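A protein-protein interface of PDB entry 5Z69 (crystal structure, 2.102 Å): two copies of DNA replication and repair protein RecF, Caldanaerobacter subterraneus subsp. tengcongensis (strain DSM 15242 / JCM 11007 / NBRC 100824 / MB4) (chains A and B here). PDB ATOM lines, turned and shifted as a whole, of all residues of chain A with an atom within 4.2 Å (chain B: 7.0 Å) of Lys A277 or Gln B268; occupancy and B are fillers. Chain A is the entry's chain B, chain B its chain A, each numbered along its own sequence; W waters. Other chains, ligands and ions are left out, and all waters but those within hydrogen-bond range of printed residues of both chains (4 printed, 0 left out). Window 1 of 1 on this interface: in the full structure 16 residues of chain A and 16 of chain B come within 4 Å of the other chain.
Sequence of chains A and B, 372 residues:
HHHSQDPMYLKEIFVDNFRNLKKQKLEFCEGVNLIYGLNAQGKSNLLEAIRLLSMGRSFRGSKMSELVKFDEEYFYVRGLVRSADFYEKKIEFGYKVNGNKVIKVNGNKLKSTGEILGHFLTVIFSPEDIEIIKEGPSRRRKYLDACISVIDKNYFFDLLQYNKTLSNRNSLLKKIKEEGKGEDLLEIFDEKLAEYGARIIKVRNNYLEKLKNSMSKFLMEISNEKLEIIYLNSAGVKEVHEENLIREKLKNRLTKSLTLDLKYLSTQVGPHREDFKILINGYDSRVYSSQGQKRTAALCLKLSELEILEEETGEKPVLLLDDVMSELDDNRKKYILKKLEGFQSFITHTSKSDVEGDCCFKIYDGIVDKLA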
ATOM      1  N   GLU A 228       1.493  11.738 -24.199  1.00  0.00           N
ATOM      2  CA  GLU A 228       0.750  12.759 -23.480  1.00  0.00           C
ATOM      3  C   GLU A 228       1.601  13.405 -22.373  1.00  0.00           C
ATOM      4  O   GLU A 228       2.477  12.761 -21.800  1.00  0.00           O
ATOM      5  CB  GLU A 228      -0.536  12.159 -22.896  1.00  0.00           C
ATOM      6  CG  GLU A 228      -1.492  11.613 -23.969  1.00  0.00           C
ATOM      7  CD  GLU A 228      -1.316  10.117 -24.300  1.00  0.00           C
ATOM      8  OE1 GLU A 228      -0.435   9.411 -23.736  1.00  0.00           O
ATOM      9  OE2 GLU A 228      -2.098   9.644 -25.145  1.00  0.00           O
ATOM     10  N   ILE A 229       1.367  14.694 -22.117  1.00  0.00           N
ATOM     11  CA  ILE A 229       1.984  15.368 -20.967  1.00  0.00           C
ATOM     12  C   ILE A 229       0.909  15.871 -20.035  1.00  0.00           C
ATOM     13  O   ILE A 229      -0.065  16.484 -20.468  1.00  0.00           O
ATOM     14  CB  ILE A 229       2.868  16.589 -21.348  1.00  0.00           C
ATOM     15  CG1 ILE A 229       4.316  16.193 -21.515  1.00  0.00           C
ATOM     16  CG2 ILE A 229       2.997  17.524 -20.174  1.00  0.00           C
ATOM     17  CD1 ILE A 229       4.643  15.812 -22.816  1.00  0.00           C
ATOM     18  N   ILE A 230       1.072  15.611 -18.750  1.00  0.00           N
ATOM     19  CA  ILE A 230       0.126  16.138 -17.788  1.00  0.00           C
ATOM     20  C   ILE A 230       0.884  17.068 -16.845  1.00  0.00           C
ATOM     21  O   ILE A 230       1.809  16.646 -16.124  1.00  0.00           O
ATOM     22  CB  ILE A 230      -0.625  14.991 -17.020  1.00  0.00           C
ATOM     23  CG1 ILE A 230      -1.875  14.540 -17.791  1.00  0.00           C
ATOM     24  CG2 ILE A 230      -1.184  15.502 -15.722  1.00  0.00           C
ATOM     25  CD1 ILE A 230      -1.647  13.863 -19.114  1.00  0.00           C
ATOM     26  N   PHE A 276       5.686  17.208 -14.071  1.00  0.00           N
ATOM     27  CA  PHE A 276       4.794  16.870 -15.163  1.00  0.00           C
ATOM     28  C   PHE A 276       5.012  15.424 -15.540  1.00  0.00           C
ATOM     29  O   PHE A 276       6.135  14.915 -15.498  1.00  0.00           O
ATOM     30  CB  PHE A 276       4.976  17.798 -16.389  1.00  0.00           C
ATOM     31  CG  PHE A 276       6.380  17.843 -16.947  1.00  0.00           C
ATOM     32  CD1 PHE A 276       7.315  18.711 -16.423  1.00  0.00           C
ATOM     33  CD2 PHE A 276       6.744  17.042 -18.021  1.00  0.00           C
ATOM     34  CE1 PHE A 276       8.615  18.775 -16.961  1.00  0.00           C
ATOM     35  CE2 PHE A 276       8.016  17.085 -18.552  1.00  0.00           C
ATOM     36  CZ  PHE A 276       8.962  17.958 -18.026  1.00  0.00           C
ATOM     37  N   LYS A 277       3.917  14.759 -15.892  1.00  0.00           N
ATOM     38  CA  LYS A 277       3.974  13.361 -16.248  1.00  0.00           C
ATOM     39  C   LYS A 277       4.204  13.184 -17.721  1.00  0.00           C
ATOM     40  O   LYS A 277       3.602  13.880 -18.539  1.00  0.00           O
ATOM     41  CB  LYS A 277       2.675  12.644 -15.873  1.00  0.00           C
ATOM     42  CG  LYS A 277       2.543  12.322 -14.403  1.00  0.00           C
ATOM     43  CD  LYS A 277       1.371  11.376 -14.168  1.00  0.00           C
ATOM     44  CE  LYS A 277       0.245  12.076 -13.460  1.00  0.00           C
ATOM     45  NZ  LYS A 277      -0.403  11.189 -12.451  1.00  0.00           N
ATOM     46  N   ILE A 278       5.029  12.208 -18.059  1.00  0.00           N
ATOM     47  CA  ILE A 278       5.252  11.879 -19.449  1.00  0.00           C
ATOM     48  C   ILE A 278       4.680  10.503 -19.729  1.00  0.00           C
ATOM     49  O   ILE A 278       5.225   9.498 -19.277  1.00  0.00           O
ATOM     50  CB  ILE A 278       6.735  11.908 -19.802  1.00  0.00           C
ATOM     51  CG1 ILE A 278       7.313  13.288 -19.478  1.00  0.00           C
ATOM     52  CG2 ILE A 278       6.918  11.537 -21.263  1.00  0.00           C
ATOM     53  CD1 ILE A 278       8.818  13.365 -19.661  1.00  0.00           C
ATOM     54  N   LEU A 279       3.592  10.480 -20.490  1.00  0.00           N
ATOM     55  CA  LEU A 279       2.813   9.271 -20.702  1.00  0.00           C
ATOM     56  C   LEU A 279       2.912   8.739 -22.122  1.00  0.00           C
ATOM     57  O   LEU A 279       2.790   9.492 -23.091  1.00  0.00           O
ATOM     58  CB  LEU A 279       1.354   9.533 -20.379  1.00  0.00           C
ATOM     59  CG  LEU A 279       1.075  10.284 -19.082  1.00  0.00           C
ATOM     60  CD1 LEU A 279      -0.426  10.442 -18.924  1.00  0.00           C
ATOM     61  CD2 LEU A 279       1.697   9.570 -17.882  1.00  0.00           C
ATOM     62  N   GLY A 282      -1.029   6.441 -22.630  1.00  0.00           N
ATOM     63  CA  GLY A 282      -1.816   6.579 -21.421  1.00  0.00           C
ATOM     64  C   GLY A 282      -1.162   6.060 -20.154  1.00  0.00           C
ATOM     65  O   GLY A 282      -1.704   6.232 -19.060  1.00  0.00           O
ATOM     66  N   ASP A 284       2.192   5.868 -17.475  1.00  0.00           N
ATOM     67  CA  ASP A 284       3.337   6.625 -16.989  1.00  0.00           C
ATOM     68  C   ASP A 284       4.653   5.974 -17.394  1.00  0.00           C
ATOM     69  O   ASP A 284       4.904   4.822 -17.036  1.00  0.00           O
ATOM     70  CB  ASP A 284       3.275   6.783 -15.468  1.00  0.00           C
ATOM     71  CG  ASP A 284       4.209   7.871 -14.973  1.00  0.00           C
ATOM     72  OD1 ASP A 284       5.272   8.038 -15.593  1.00  0.00           O
ATOM     73  OD2 ASP A 284       3.876   8.573 -13.996  1.00  0.00           O
ATOM     74  N   LEU B 166     -13.818   2.716  -8.645  1.00  0.00           N
ATOM     75  CA  LEU B 166     -13.077   2.833  -9.886  1.00  0.00           C
ATOM     76  C   LEU B 166     -13.928   2.357 -11.066  1.00  0.00           C
ATOM     77  O   LEU B 166     -14.013   3.026 -12.107  1.00  0.00           O
ATOM     78  CB  LEU B 166     -11.789   2.031  -9.804  1.00  0.00           C
ATOM     79  CG  LEU B 166     -10.959   2.016 -11.081  1.00  0.00           C
ATOM     80  CD1 LEU B 166     -10.502   3.436 -11.404  1.00  0.00           C
ATOM     81  CD2 LEU B 166      -9.753   1.089 -10.943  1.00  0.00           C
ATOM     82  N   ARG B 169     -16.501   4.840 -11.847  1.00  0.00           N
ATOM     83  CA  ARG B 169     -15.948   6.005 -12.502  1.00  0.00           C
ATOM     84  C   ARG B 169     -15.709   5.697 -13.977  1.00  0.00           C
ATOM     85  O   ARG B 169     -16.045   6.498 -14.848  1.00  0.00           O
ATOM     86  CB  ARG B 169     -14.648   6.467 -11.838  1.00  0.00           C
ATOM     87  CG  ARG B 169     -14.149   7.816 -12.397  1.00  0.00           C
ATOM     88  CD  ARG B 169     -12.736   8.124 -11.975  1.00  0.00           C
ATOM     89  NE  ARG B 169     -12.334   9.504 -12.249  1.00  0.00           N
ATOM     90  CZ  ARG B 169     -11.601   9.883 -13.294  1.00  0.00           C
ATOM     91  NH1 ARG B 169     -11.186   8.993 -14.191  1.00  0.00           N
ATOM     92  NH2 ARG B 169     -11.286  11.157 -13.440  1.00  0.00           N
ATOM     93  N   ASN B 170     -15.149   4.527 -14.263  1.00  0.00           N
ATOM     94  CA  ASN B 170     -14.829   4.181 -15.642  1.00  0.00           C
ATOM     95  C   ASN B 170     -16.052   4.044 -16.550  1.00  0.00           C
ATOM     96  O   ASN B 170     -16.016   4.414 -17.721  1.00  0.00           O
ATOM     97  CB  ASN B 170     -14.011   2.900 -15.670  1.00  0.00           C
ATOM     98  CG  ASN B 170     -12.582   3.141 -15.257  1.00  0.00           C
ATOM     99  OD1 ASN B 170     -12.094   4.272 -15.341  1.00  0.00           O
ATOM    100  ND2 ASN B 170     -11.901   2.097 -14.804  1.00  0.00           N
ATOM    101  N   SER B 234       1.101   6.554  -6.447  1.00  0.00           N
ATOM    102  CA  SER B 234       0.415   7.371  -7.445  1.00  0.00           C
ATOM    103  C   SER B 234       0.247   8.818  -6.986  1.00  0.00           C
ATOM    104  O   SER B 234      -0.236   9.661  -7.744  1.00  0.00           O
ATOM    105  CB  SER B 234      -0.952   6.772  -7.777  1.00  0.00           C
ATOM    106  OG  SER B 234      -1.620   6.337  -6.600  1.00  0.00           O
ATOM    107  N   ARG B 253      -4.481  15.229  -9.044  1.00  0.00           N
ATOM    108  CA  ARG B 253      -4.092  14.445 -10.190  1.00  0.00           C
ATOM    109  C   ARG B 253      -5.291  13.907 -10.962  1.00  0.00           C
ATOM    110  O   ARG B 253      -5.254  13.899 -12.182  1.00  0.00           O
ATOM    111  CB  ARG B 253      -3.162  13.322  -9.738  1.00  0.00           C
ATOM    112  CG  ARG B 253      -1.869  13.871  -9.201  1.00  0.00           C
ATOM    113  CD  ARG B 253      -0.980  12.839  -8.549  1.00  0.00           C
ATOM    114  NE  ARG B 253       0.333  13.427  -8.313  1.00  0.00           N
ATOM    115  CZ  ARG B 253       1.486  12.822  -8.565  1.00  0.00           C
ATOM    116  NH1 ARG B 253       1.494  11.581  -9.035  1.00  0.00           N
ATOM    117  NH2 ARG B 253       2.630  13.460  -8.333  1.00  0.00           N
ATOM    118  N   LEU B 254      -6.344  13.472 -10.268  1.00  0.00           N
ATOM    119  CA  LEU B 254      -7.557  12.984 -10.932  1.00  0.00           C
ATOM    120  C   LEU B 254      -8.165  14.084 -11.798  1.00  0.00           C
ATOM    121  O   LEU B 254      -8.563  13.859 -12.952  1.00  0.00           O
ATOM    122  CB  LEU B 254      -8.607  12.508  -9.905  1.00  0.00           C
ATOM    123  CG  LEU B 254      -8.285  11.296  -9.043  1.00  0.00           C
ATOM    124  CD1 LEU B 254      -9.293  11.096  -7.928  1.00  0.00           C
ATOM    125  CD2 LEU B 254      -8.276  10.105  -9.957  1.00  0.00           C
ATOM    126  N   SER B 257      -6.466  14.846 -14.940  1.00  0.00           N
ATOM    127  CA  SER B 257      -6.369  13.682 -15.808  1.00  0.00           C
ATOM    128  C   SER B 257      -7.582  13.541 -16.725  1.00  0.00           C
ATOM    129  O   SER B 257      -7.649  12.634 -17.560  1.00  0.00           O
ATOM    130  CB  SER B 257      -6.204  12.415 -14.950  1.00  0.00           C
ATOM    131  OG  SER B 257      -5.847  11.301 -15.742  1.00  0.00           O
ATOM    132  N   LEU B 260      -7.344  13.169 -20.625  1.00  0.00           N
ATOM    133  CA  LEU B 260      -6.671  11.909 -20.905  1.00  0.00           C
ATOM    134  C   LEU B 260      -7.582  10.710 -20.637  1.00  0.00           C
ATOM    135  O   LEU B 260      -7.632   9.764 -21.436  1.00  0.00           O
ATOM    136  CB  LEU B 260      -5.400  11.778 -20.067  1.00  0.00           C
ATOM    137  CG  LEU B 260      -4.704  10.435 -20.275  1.00  0.00           C
ATOM    138  CD1 LEU B 260      -3.711  10.521 -21.426  1.00  0.00           C
ATOM    139  CD2 LEU B 260      -4.026   9.961 -18.999  1.00  0.00           C
ATOM    140  N   ASP B 261      -8.306  10.756 -19.519  1.00  0.00           N
ATOM    141  CA  ASP B 261      -9.162   9.628 -19.131  1.00  0.00           C
ATOM    142  C   ASP B 261     -10.329   9.452 -20.103  1.00  0.00           C
ATOM    143  O   ASP B 261     -10.746   8.328 -20.409  1.00  0.00           O
ATOM    144  CB  ASP B 261      -9.672   9.823 -17.700  1.00  0.00           C
ATOM    145  CG  ASP B 261      -8.568   9.634 -16.656  1.00  0.00           C
ATOM    146  OD1 ASP B 261      -7.470   9.143 -17.013  1.00  0.00           O
ATOM    147  OD2 ASP B 261      -8.800   9.967 -15.478  1.00  0.00           O
ATOM    148  N   SER B 266     -10.341   5.194 -19.341  1.00  0.00           N
ATOM    149  CA  SER B 266      -9.785   4.547 -18.146  1.00  0.00           C
ATOM    150  C   SER B 266      -9.287   5.608 -17.170  1.00  0.00           C
ATOM    151  O   SER B 266      -9.346   6.801 -17.454  1.00  0.00           O
ATOM    152  CB  SER B 266      -8.644   3.605 -18.514  1.00  0.00           C
ATOM    153  OG  SER B 266      -7.509   4.361 -18.924  1.00  0.00           O
ATOM    154  N   THR B 267      -8.788   5.174 -16.020  1.00  0.00           N
ATOM    155  CA  THR B 267      -8.334   6.098 -14.988  1.00  0.00           C
ATOM    156  C   THR B 267      -6.850   5.896 -14.781  1.00  0.00           C
ATOM    157  O   THR B 267      -6.460   4.853 -14.263  1.00  0.00           O
ATOM    158  CB  THR B 267      -9.084   5.864 -13.642  1.00  0.00           C
ATOM    159  OG1 THR B 267     -10.488   6.027 -13.841  1.00  0.00           O
ATOM    160  CG2 THR B 267      -8.618   6.850 -12.571  1.00  0.00           C
ATOM    161  N   GLN B 268      -6.005   6.856 -15.182  1.00  0.00           N
ATOM    162  CA  GLN B 268      -4.560   6.623 -15.038  1.00  0.00           C
ATOM    163  C   GLN B 268      -4.056   6.924 -13.619  1.00  0.00           C
ATOM    164  O   GLN B 268      -2.938   6.540 -13.258  1.00  0.00           O
ATOM    165  CB  GLN B 268      -3.752   7.428 -16.092  1.00  0.00           C
ATOM    166  CG  GLN B 268      -3.182   8.719 -15.618  1.00  0.00           C
ATOM    167  CD  GLN B 268      -1.838   8.632 -14.891  1.00  0.00           C
ATOM    168  OE1 GLN B 268      -1.529   9.518 -14.118  1.00  0.00           O
ATOM    169  NE2 GLN B 268      -1.056   7.588 -15.126  1.00  0.00           N
ATOM    170  N   VAL B 269      -4.873   7.587 -12.800  1.00  0.00           N
ATOM    171  CA  VAL B 269      -4.441   7.951 -11.457  1.00  0.00           C
ATOM    172  C   VAL B 269      -4.950   6.992 -10.366  1.00  0.00           C
ATOM    173  O   VAL B 269      -6.146   6.830 -10.188  1.00  0.00           O
ATOM    174  CB  VAL B 269      -4.905   9.362 -11.075  1.00  0.00           C
ATOM    175  CG1 VAL B 269      -4.616   9.627  -9.615  1.00  0.00           C
ATOM    176  CG2 VAL B 269      -4.206  10.437 -11.952  1.00  0.00           C
ATOM    177  N   GLY B 270      -4.045   6.388  -9.614  1.00  0.00           N
ATOM    178  CA  GLY B 270      -4.464   5.660  -8.424  1.00  0.00           C
ATOM    179  C   GLY B 270      -3.633   4.431  -8.129  1.00  0.00           C
ATOM    180  O   GLY B 270      -2.723   4.092  -8.906  1.00  0.00           O
ATOM    181  N   PRO B 271      -3.944   3.749  -7.001  1.00  0.00           N
ATOM    182  CA  PRO B 271      -3.288   2.515  -6.565  1.00  0.00           C
ATOM    183  C   PRO B 271      -3.192   1.444  -7.643  1.00  0.00           C
ATOM    184  O   PRO B 271      -2.257   0.650  -7.608  1.00  0.00           O
ATOM    185  CB  PRO B 271      -4.187   2.029  -5.411  1.00  0.00           C
ATOM    186  CG  PRO B 271      -4.766   3.258  -4.839  1.00  0.00           C
ATOM    187  CD  PRO B 271      -4.808   4.312  -5.944  1.00  0.00           C
ATOM    188  N   HIS B 272      -4.128   1.430  -8.589  1.00  0.00           N
ATOM    189  CA  HIS B 272      -4.165   0.378  -9.607  1.00  0.00           C
ATOM    190  C   HIS B 272      -3.145   0.579 -10.725  1.00  0.00           C
ATOM    191  O   HIS B 272      -3.099  -0.220 -11.671  1.00  0.00           O
ATOM    192  CB  HIS B 272      -5.567   0.277 -10.221  1.00  0.00           C
ATOM    193  CG  HIS B 272      -5.994   1.527 -10.924  1.00  0.00           C
ATOM    194  ND1 HIS B 272      -6.342   2.677 -10.249  1.00  0.00           N
ATOM    195  CD2 HIS B 272      -6.102   1.818 -12.243  1.00  0.00           C
ATOM    196  CE1 HIS B 272      -6.662   3.618 -11.120  1.00  0.00           C
ATOM    197  NE2 HIS B 272      -6.532   3.120 -12.336  1.00  0.00           N
ATOM    198  N   ARG B 273      -2.340   1.639 -10.629  1.00  0.00           N
ATOM    199  CA  ARG B 273      -1.279   1.868 -11.614  1.00  0.00           C
ATOM    200  C   ARG B 273       0.076   1.936 -10.962  1.00  0.00           C
ATOM    201  O   ARG B 273       1.029   2.345 -11.599  1.00  0.00           O
ATOM    202  CB  ARG B 273      -1.500   3.173 -12.395  1.00  0.00           C
ATOM    203  CG  ARG B 273      -2.706   3.163 -13.307  1.00  0.00           C
ATOM    204  CD  ARG B 273      -2.492   2.211 -14.465  1.00  0.00           C
ATOM    205  NE  ARG B 273      -3.556   2.347 -15.456  1.00  0.00           N
ATOM    206  CZ  ARG B 273      -3.586   3.282 -16.402  1.00  0.00           C
ATOM    207  NH2 ARG B 273      -4.614   3.304 -17.240  1.00  0.00           N
ATOM    208  N   GLU B 274       0.162   1.557  -9.690  1.00  0.00           N
ATOM    209  CA  GLU B 274       1.411   1.708  -8.944  1.00  0.00           C
ATOM    210  C   GLU B 274       2.358   0.536  -9.162  1.00  0.00           C
ATOM    211  O   GLU B 274       1.994  -0.466  -9.783  1.00  0.00           O
ATOM    212  CB  GLU B 274       1.115   1.885  -7.449  1.00  0.00           C
ATOM    213  CG  GLU B 274       0.292   3.138  -7.147  1.00  0.00           C
ATOM    214  CD  GLU B 274       0.041   3.353  -5.660  1.00  0.00           C
ATOM    215  OE1 GLU B 274       0.280   2.419  -4.864  1.00  0.00           O
ATOM    216  OE2 GLU B 274      -0.395   4.464  -5.284  1.00  0.00           O
HETATM  217  O   HOH W   1      -1.048   9.451 -10.349  1.00  0.00           O
HETATM  218  O   HOH W   2      -2.666  12.992 -13.351  1.00  0.00           O
HETATM  219  O   HOH W   3       0.177   4.620 -15.530  1.00  0.00           O
HETATM  220  O   HOH W   4      -4.300   5.675 -18.930  1.00  0.00           O
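The side-chain amide oxygen (OE1) of Gln B268 sits at hydrogen-bond distance from the side-chain amino group (NZ) of Lys A277, at 2.6 Å.
N of Glu A228 lies within hydrogen-bond range of O of Leu A279, at 2.8 Å. OE1 of Glu A228 is in hydrogen-bond range of N of Gly A282. The backbone NH (N) of Lys A277 is in hydrogen-bond range of the backbone carbonyl oxygen (O) of Ile A230. The side-chain carboxylate (OD1) of Asp B261 sits at hydrogen-bond distance from the backbone NH (N) of Gln B268, 3.3 Å away. NH1 of Arg B253 lies within hydrogen-bond range of O of Ser B234 (2.9 Å).
Among the printed residues, pairs that only touch across the chains: Glu A228 with Leu B260, Leu A279 with Leu B260, Gly A282 with Gln B268, Lys A277 with Val B269 and Lys A277 with Arg B253.
Printed residues of chain B within 4 Å of Glu A228: Leu B260 (3.5 Å). Ile A230 touches none of the printed residues of chain B. Printed residues of chain B within 4 Å of Lys A277: Arg B253 (3.9 Å), Gln B268 (2.6 Å) and Val B269 (3.9 Å). Of the printed residues of chain B, Leu A279 touches Leu B260 (3.6 Å). Printed residues of chain A within 4 Å of Arg B253: Lys A277 (3.9 Å). Of the printed residues of chain A, Leu B260 touches Glu A228 (3.5 Å) and Leu A279 (3.6 Å). Printed residues of chain A within 4 Å of Gln B268: Lys A277 and Gly A282. His B272 touches none of the printed residues of chain A. The nearest residue of chain B that does not touch Lys A277 is Ser B234 (5.0 Å). The nearest printed residue of chain A that does not touch Arg B253 is Ile A230 (5.6 Å).
Hydrophobic or aromatic side chains of chain B that line the printed part of chain A: Leu B260 and Val B269. Of the 9 printed residues of chain A, 4 touch a printed residue of chain B. Hydrophobic or aromatic side chains of chain A within 4 Å of the printed part of chain B: Leu A279. Among the printed residues, 6 pairs touch across the chains. Among the printed residues, no Asp or Glu carboxylate lies within 4 Å of a Lys or Arg side-chain nitrogen of the other chain.
No position is printed for both chains.
Water W4 lies within hydrogen-bond range of O of Gly A282 (2.7 Å), NH2 of Arg B273 (2.9 Å) and OG of Ser B266 (3.5 Å). Water W1 bridges the backbone carbonyl oxygen (O) of Ser B234 and the side-chain amino group (NZ) of Lys A277. Water W2 bridges O of Arg B253 (3.0 Å) and NZ of Lys A277 (3.0 Å). Water W3 bridges the backbone NH (N) of Asp A284 (3.1 Å) and the side-chain amide nitrogen (NE2) of Gln B268 (3.2 Å).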
